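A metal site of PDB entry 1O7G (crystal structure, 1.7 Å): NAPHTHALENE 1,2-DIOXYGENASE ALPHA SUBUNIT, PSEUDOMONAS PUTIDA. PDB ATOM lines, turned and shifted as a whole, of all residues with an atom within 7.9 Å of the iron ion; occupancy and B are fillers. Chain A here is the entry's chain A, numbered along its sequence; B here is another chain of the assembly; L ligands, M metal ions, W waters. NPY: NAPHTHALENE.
O of Trp 358 sits close to ND1 of His 213 (3.4 Å).
A ring nitrogen (ND1) of His 213 is in hydrogen-bond range of the side-chain carboxylate (OD1) of Asp 361.
OD1 of Asn 201 sits close to NE2 of His 208, at 3.5 Å.
ND1 of His 208 is in hydrogen-bond range of O of Asp 205, at 2.7 Å.
The side-chain amide oxygen (OD1) of Asn 201 lies close to the side-chain carboxylate (OD1) of Asp 205 (3.5 Å).
The side-chain amide oxygen (OD1) of Asn 201 is in hydrogen-bond range of the side-chain hydroxyl (OH) of Tyr 103 of chain B, at 3.1 Å.
ND2 of Asn 201 touches the iron ion (3.8 Å).
Four residues have an atom within 4 Å of the iron ion: Asn 201, His 208, His 213 and Asp 362.
The iron ion is bound by a ring nitrogen (NE2) of His 213 (2.0 Å), water W1 (2.1 Å), a ring nitrogen (NE2) of His 208 (2.1 Å), the side-chain carboxylate (OD2) of Asp 362 (2.3 Å) and the side-chain carboxylate (OD1) of Asp 362 (2.4 Å).
The iron ion has five donor atoms within binding distance.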
ATOM      1  N   ASN A 201       8.192  15.630   4.394  1.00  0.00           N
ATOM      2  CA  ASN A 201       8.937  15.231   5.593  1.00  0.00           C
ATOM      3  C   ASN A 201       8.424  15.983   6.801  1.00  0.00           C
ATOM      4  O   ASN A 201       8.172  15.400   7.868  1.00  0.00           O
ATOM      5  CB  ASN A 201      10.412  15.522   5.337  1.00  0.00           C
ATOM      6  CG  ASN A 201      11.306  15.194   6.515  1.00  0.00           C
ATOM      7  OD1 ASN A 201      11.723  14.034   6.678  1.00  0.00           O
ATOM      8  ND2 ASN A 201      11.608  16.181   7.322  1.00  0.00           N
ATOM      9  N   PHE A 202       8.200  17.290   6.628  1.00  0.00           N
ATOM     10  CA  PHE A 202       7.736  18.091   7.734  1.00  0.00           C
ATOM     11  C   PHE A 202       6.269  17.887   8.009  1.00  0.00           C
ATOM     12  O   PHE A 202       5.849  18.082   9.141  1.00  0.00           O
ATOM     13  CB  PHE A 202       7.962  19.578   7.512  1.00  0.00           C
ATOM     14  CG  PHE A 202       9.322  20.037   7.919  1.00  0.00           C
ATOM     15  CD1 PHE A 202      10.447  19.593   7.253  1.00  0.00           C
ATOM     16  CD2 PHE A 202       9.494  20.938   8.917  1.00  0.00           C
ATOM     17  CE1 PHE A 202      11.681  19.995   7.635  1.00  0.00           C
ATOM     18  CE2 PHE A 202      10.759  21.360   9.299  1.00  0.00           C
ATOM     19  CZ  PHE A 202      11.837  20.857   8.661  1.00  0.00           C
ATOM     20  N   ASP A 205       6.310  13.273   8.954  1.00  0.00           N
ATOM     21  CA  ASP A 205       7.287  12.259   9.123  1.00  0.00           C
ATOM     22  C   ASP A 205       7.942  12.220  10.496  1.00  0.00           C
ATOM     23  O   ASP A 205       9.058  12.710  10.691  1.00  0.00           O
ATOM     24  CB  ASP A 205       8.363  12.373   8.056  1.00  0.00           C
ATOM     25  CG  ASP A 205       9.229  11.147   7.948  1.00  0.00           C
ATOM     26  OD1 ASP A 205       9.930  11.073   6.911  1.00  0.00           O
ATOM     27  OD2 ASP A 205       9.341  10.252   8.848  1.00  0.00           O
ATOM     28  N   HIS A 208      11.010   9.060  10.733  1.00  0.00           N
ATOM     29  CA  HIS A 208      12.447   9.195  10.405  1.00  0.00           C
ATOM     30  C   HIS A 208      13.325   9.724  11.541  1.00  0.00           C
ATOM     31  O   HIS A 208      14.541   9.537  11.553  1.00  0.00           O
ATOM     32  CB  HIS A 208      12.628  10.091   9.135  1.00  0.00           C
ATOM     33  CG  HIS A 208      12.692  11.551   9.418  1.00  0.00           C
ATOM     34  ND1 HIS A 208      11.610  12.292   9.884  1.00  0.00           N
ATOM     35  CD2 HIS A 208      13.732  12.410   9.332  1.00  0.00           C
ATOM     36  CE1 HIS A 208      12.008  13.549  10.050  1.00  0.00           C
ATOM     37  NE2 HIS A 208      13.287  13.647   9.740  1.00  0.00           N
ATOM     38  N   VAL A 209      12.713  10.369  12.534  1.00  0.00           N
ATOM     39  CA  VAL A 209      13.454  11.161  13.483  1.00  0.00           C
ATOM     40  C   VAL A 209      14.509  10.366  14.215  1.00  0.00           C
ATOM     41  O   VAL A 209      15.705  10.704  14.185  1.00  0.00           O
ATOM     42  CB  VAL A 209      12.521  11.892  14.437  1.00  0.00           C
ATOM     43  CG1 VAL A 209      13.319  12.608  15.546  1.00  0.00           C
ATOM     44  CG2 VAL A 209      11.727  12.907  13.645  1.00  0.00           C
ATOM     45  N   THR A 212      17.196   8.868  11.158  1.00  0.00           N
ATOM     46  CA  THR A 212      17.892   9.954  10.433  1.00  0.00           C
ATOM     47  C   THR A 212      18.670  10.841  11.351  1.00  0.00           C
ATOM     48  O   THR A 212      19.826  11.180  11.054  1.00  0.00           O
ATOM     49  CB  THR A 212      16.906  10.827   9.668  1.00  0.00           C
ATOM     50  OG1 THR A 212      16.454  10.157   8.511  1.00  0.00           O
ATOM     51  CG2 THR A 212      17.575  12.093   9.088  1.00  0.00           C
ATOM     52  N   HIS A 213      18.072  11.211  12.502  1.00  0.00           N
ATOM     53  CA  HIS A 213      18.656  12.216  13.376  1.00  0.00           C
ATOM     54  C   HIS A 213      19.303  11.606  14.624  1.00  0.00           C
ATOM     55  O   HIS A 213      19.517  12.334  15.604  1.00  0.00           O
ATOM     56  CB  HIS A 213      17.619  13.272  13.805  1.00  0.00           C
ATOM     57  CG  HIS A 213      17.044  14.074  12.657  1.00  0.00           C
ATOM     58  ND1 HIS A 213      17.782  14.995  11.948  1.00  0.00           N
ATOM     59  CD2 HIS A 213      15.815  14.051  12.073  1.00  0.00           C
ATOM     60  CE1 HIS A 213      17.028  15.519  10.992  1.00  0.00           C
ATOM     61  NE2 HIS A 213      15.828  14.975  11.056  1.00  0.00           N
ATOM     62  N   LEU A 307       8.039  24.005  12.660  1.00  0.00           N
ATOM     63  CA  LEU A 307       8.078  23.204  13.901  1.00  0.00           C
ATOM     64  C   LEU A 307       7.757  24.182  15.002  1.00  0.00           C
ATOM     65  O   LEU A 307       8.576  25.044  15.342  1.00  0.00           O
ATOM     66  CB  LEU A 307       9.445  22.581  14.168  1.00  0.00           C
ATOM     67  CG  LEU A 307      10.094  21.714  13.092  1.00  0.00           C
ATOM     68  CD1 LEU A 307      11.437  21.224  13.523  1.00  0.00           C
ATOM     69  CD2 LEU A 307       9.195  20.587  12.683  1.00  0.00           C
ATOM     70  N   PHE A 352      18.591  23.941  12.446  1.00  0.00           N
ATOM     71  CA  PHE A 352      17.897  23.836  11.170  1.00  0.00           C
ATOM     72  C   PHE A 352      18.264  24.860  10.085  1.00  0.00           C
ATOM     73  O   PHE A 352      17.682  24.833   9.020  1.00  0.00           O
ATOM     74  CB  PHE A 352      16.370  23.814  11.448  1.00  0.00           C
ATOM     75  CG  PHE A 352      15.877  22.467  11.788  1.00  0.00           C
ATOM     76  CD1 PHE A 352      15.497  21.578  10.804  1.00  0.00           C
ATOM     77  CD2 PHE A 352      15.889  22.028  13.082  1.00  0.00           C
ATOM     78  CE1 PHE A 352      15.087  20.299  11.096  1.00  0.00           C
ATOM     79  CE2 PHE A 352      15.495  20.735  13.395  1.00  0.00           C
ATOM     80  CZ  PHE A 352      15.083  19.868  12.430  1.00  0.00           C
ATOM     81  N   TRP A 358      20.959  19.371  12.549  1.00  0.00           N
ATOM     82  CA  TRP A 358      19.829  18.481  12.270  1.00  0.00           C
ATOM     83  C   TRP A 358      19.449  18.464  10.781  1.00  0.00           C
ATOM     84  O   TRP A 358      19.297  17.412  10.178  1.00  0.00           O
ATOM     85  CB  TRP A 358      18.572  18.864  13.079  1.00  0.00           C
ATOM     86  CG  TRP A 358      18.664  18.697  14.553  1.00  0.00           C
ATOM     87  CD1 TRP A 358      19.492  19.323  15.428  1.00  0.00           C
ATOM     88  CD2 TRP A 358      17.779  17.907  15.351  1.00  0.00           C
ATOM     89  NE1 TRP A 358      19.209  18.949  16.730  1.00  0.00           N
ATOM     90  CE2 TRP A 358      18.159  18.058  16.693  1.00  0.00           C
ATOM     91  CE3 TRP A 358      16.698  17.063  15.047  1.00  0.00           C
ATOM     92  CZ2 TRP A 358      17.479  17.419  17.728  1.00  0.00           C
ATOM     93  CZ3 TRP A 358      16.027  16.442  16.060  1.00  0.00           C
ATOM     94  CH2 TRP A 358      16.429  16.606  17.380  1.00  0.00           C
ATOM     95  N   GLU A 359      19.274  19.619  10.198  1.00  0.00           N
ATOM     96  CA  GLU A 359      18.853  19.753   8.815  1.00  0.00           C
ATOM     97  C   GLU A 359      19.850  19.020   7.896  1.00  0.00           C
ATOM     98  O   GLU A 359      19.445  18.426   6.898  1.00  0.00           O
ATOM     99  CB  GLU A 359      18.717  21.217   8.440  1.00  0.00           C
ATOM    100  CG  GLU A 359      18.354  21.512   6.980  1.00  0.00           C
ATOM    101  CD  GLU A 359      16.884  21.843   6.735  1.00  0.00           C
ATOM    102  OE1 GLU A 359      15.997  21.408   7.509  1.00  0.00           O
ATOM    103  OE2 GLU A 359      16.597  22.527   5.694  1.00  0.00           O
ATOM    104  N   SER A 360      21.124  19.035   8.237  1.00  0.00           N
ATOM    105  CA  SER A 360      22.130  18.347   7.438  1.00  0.00           C
ATOM    106  C   SER A 360      21.896  16.843   7.390  1.00  0.00           C
ATOM    107  O   SER A 360      22.171  16.201   6.367  1.00  0.00           O
ATOM    108  CB  SER A 360      23.529  18.668   7.950  1.00  0.00           C
ATOM    109  OG  SER A 360      23.869  17.881   9.075  1.00  0.00           O
ATOM    110  N   ASP A 361      21.329  16.290   8.456  1.00  0.00           N
ATOM    111  CA  ASP A 361      21.010  14.858   8.486  1.00  0.00           C
ATOM    112  C   ASP A 361      20.020  14.502   7.380  1.00  0.00           C
ATOM    113  O   ASP A 361      20.049  13.382   6.856  1.00  0.00           O
ATOM    114  CB  ASP A 361      20.350  14.414   9.818  1.00  0.00           C
ATOM    115  CG  ASP A 361      21.214  14.660  11.044  1.00  0.00           C
ATOM    116  OD1 ASP A 361      20.639  14.803  12.156  1.00  0.00           O
ATOM    117  OD2 ASP A 361      22.457  14.686  10.942  1.00  0.00           O
ATOM    118  N   ASP A 362      19.129  15.425   7.023  1.00  0.00           N
ATOM    119  CA  ASP A 362      18.093  15.168   6.018  1.00  0.00           C
ATOM    120  C   ASP A 362      18.540  15.387   4.574  1.00  0.00           C
ATOM    121  O   ASP A 362      17.856  14.973   3.655  1.00  0.00           O
ATOM    122  CB  ASP A 362      16.875  16.084   6.241  1.00  0.00           C
ATOM    123  CG  ASP A 362      16.157  15.800   7.545  1.00  0.00           C
ATOM    124  OD1 ASP A 362      16.122  16.687   8.414  1.00  0.00           O
ATOM    125  OD2 ASP A 362      15.623  14.691   7.714  1.00  0.00           O
ATOM    126  N   ASN A 363      19.700  16.021   4.393  1.00  0.00           N
ATOM    127  CA  ASN A 363      20.146  16.355   3.027  1.00  0.00           C
ATOM    128  C   ASN A 363      20.112  15.186   2.082  1.00  0.00           C
ATOM    129  O   ASN A 363      19.452  15.217   1.034  1.00  0.00           O
ATOM    130  CB  ASN A 363      21.575  16.899   3.049  1.00  0.00           C
ATOM    131  CG  ASN A 363      21.683  18.397   3.339  1.00  0.00           C
ATOM    132  OD1 ASN A 363      22.784  18.971   3.222  1.00  0.00           O
ATOM    133  ND2 ASN A 363      20.575  19.043   3.680  1.00  0.00           N
ATOM    134  N   ASN A 365      18.786  12.228   2.371  1.00  0.00           N
ATOM    135  CA  ASN A 365      17.460  11.656   2.259  1.00  0.00           C
ATOM    136  C   ASN A 365      16.646  12.359   1.170  1.00  0.00           C
ATOM    137  O   ASN A 365      16.090  11.709   0.284  1.00  0.00           O
ATOM    138  CB  ASN A 365      16.647  11.748   3.561  1.00  0.00           C
ATOM    139  CG  ASN A 365      17.245  10.983   4.694  1.00  0.00           C
ATOM    140  OD1 ASN A 365      17.968  10.046   4.509  1.00  0.00           O
ATOM    141  ND2 ASN A 365      16.928  11.432   5.921  1.00  0.00           N
ATOM    142  N   MET A 366      16.546  13.685   1.258  1.00  0.00           N
ATOM    143  CA  MET A 366      15.738  14.432   0.312  1.00  0.00           C
ATOM    144  C   MET A 366      16.297  14.475  -1.084  1.00  0.00           C
ATOM    145  O   MET A 366      15.555  14.337  -2.071  1.00  0.00           O
ATOM    146  CB  MET A 366      15.506  15.867   0.785  1.00  0.00           C
ATOM    147  CG  MET A 366      14.923  15.986   2.195  1.00  0.00           C
ATOM    148  SD  MET A 366      13.203  15.479   2.307  1.00  0.00           S
ATOM    149  CE  MET A 366      12.670  16.400   3.736  1.00  0.00           C
ATOM    150  N   TYR B 103      17.052   6.594   6.051  1.00  0.00           N
ATOM    151  CA  TYR B 103      15.930   7.527   6.190  1.00  0.00           C
ATOM    152  C   TYR B 103      15.053   7.038   7.365  1.00  0.00           C
ATOM    153  O   TYR B 103      15.023   7.708   8.394  1.00  0.00           O
ATOM    154  CB  TYR B 103      15.181   7.628   4.858  1.00  0.00           C
ATOM    155  CG  TYR B 103      14.286   8.864   4.696  1.00  0.00           C
ATOM    156  CD1 TYR B 103      13.777   9.195   3.451  1.00  0.00           C
ATOM    157  CD2 TYR B 103      13.950   9.654   5.761  1.00  0.00           C
ATOM    158  CE1 TYR B 103      12.980  10.347   3.273  1.00  0.00           C
ATOM    159  CE2 TYR B 103      13.121  10.780   5.591  1.00  0.00           C
ATOM    160  CZ  TYR B 103      12.616  11.089   4.368  1.00  0.00           C
ATOM    161  OH  TYR B 103      11.808  12.217   4.221  1.00  0.00           O
HETATM  162  C1  NPY L   1      11.213  16.952  11.816  1.00  0.00           C
HETATM  163  C2  NPY L   1      10.323  16.575  10.796  1.00  0.00           C
HETATM  164  C3  NPY L   1       9.108  15.932  11.069  1.00  0.00           C
HETATM  165  C4  NPY L   1       8.751  15.645  12.385  1.00  0.00           C
HETATM  166  C4A NPY L   1       9.585  16.016  13.420  1.00  0.00           C
HETATM  167  C5  NPY L   1       9.218  15.768  14.751  1.00  0.00           C
HETATM  168  C6  NPY L   1      10.084  16.141  15.772  1.00  0.00           C
HETATM  169  C7  NPY L   1      11.320  16.758  15.499  1.00  0.00           C
HETATM  170  C8  NPY L   1      11.715  17.048  14.199  1.00  0.00           C
HETATM  171  C8A NPY L   1      10.873  16.689  13.132  1.00  0.00           C
HETATM  172 FE    FE M   1      14.514  15.297   9.595  1.00  0.00          FE
HETATM  173  O   HOH W   1      13.326  16.968   9.658  1.00  0.00           O
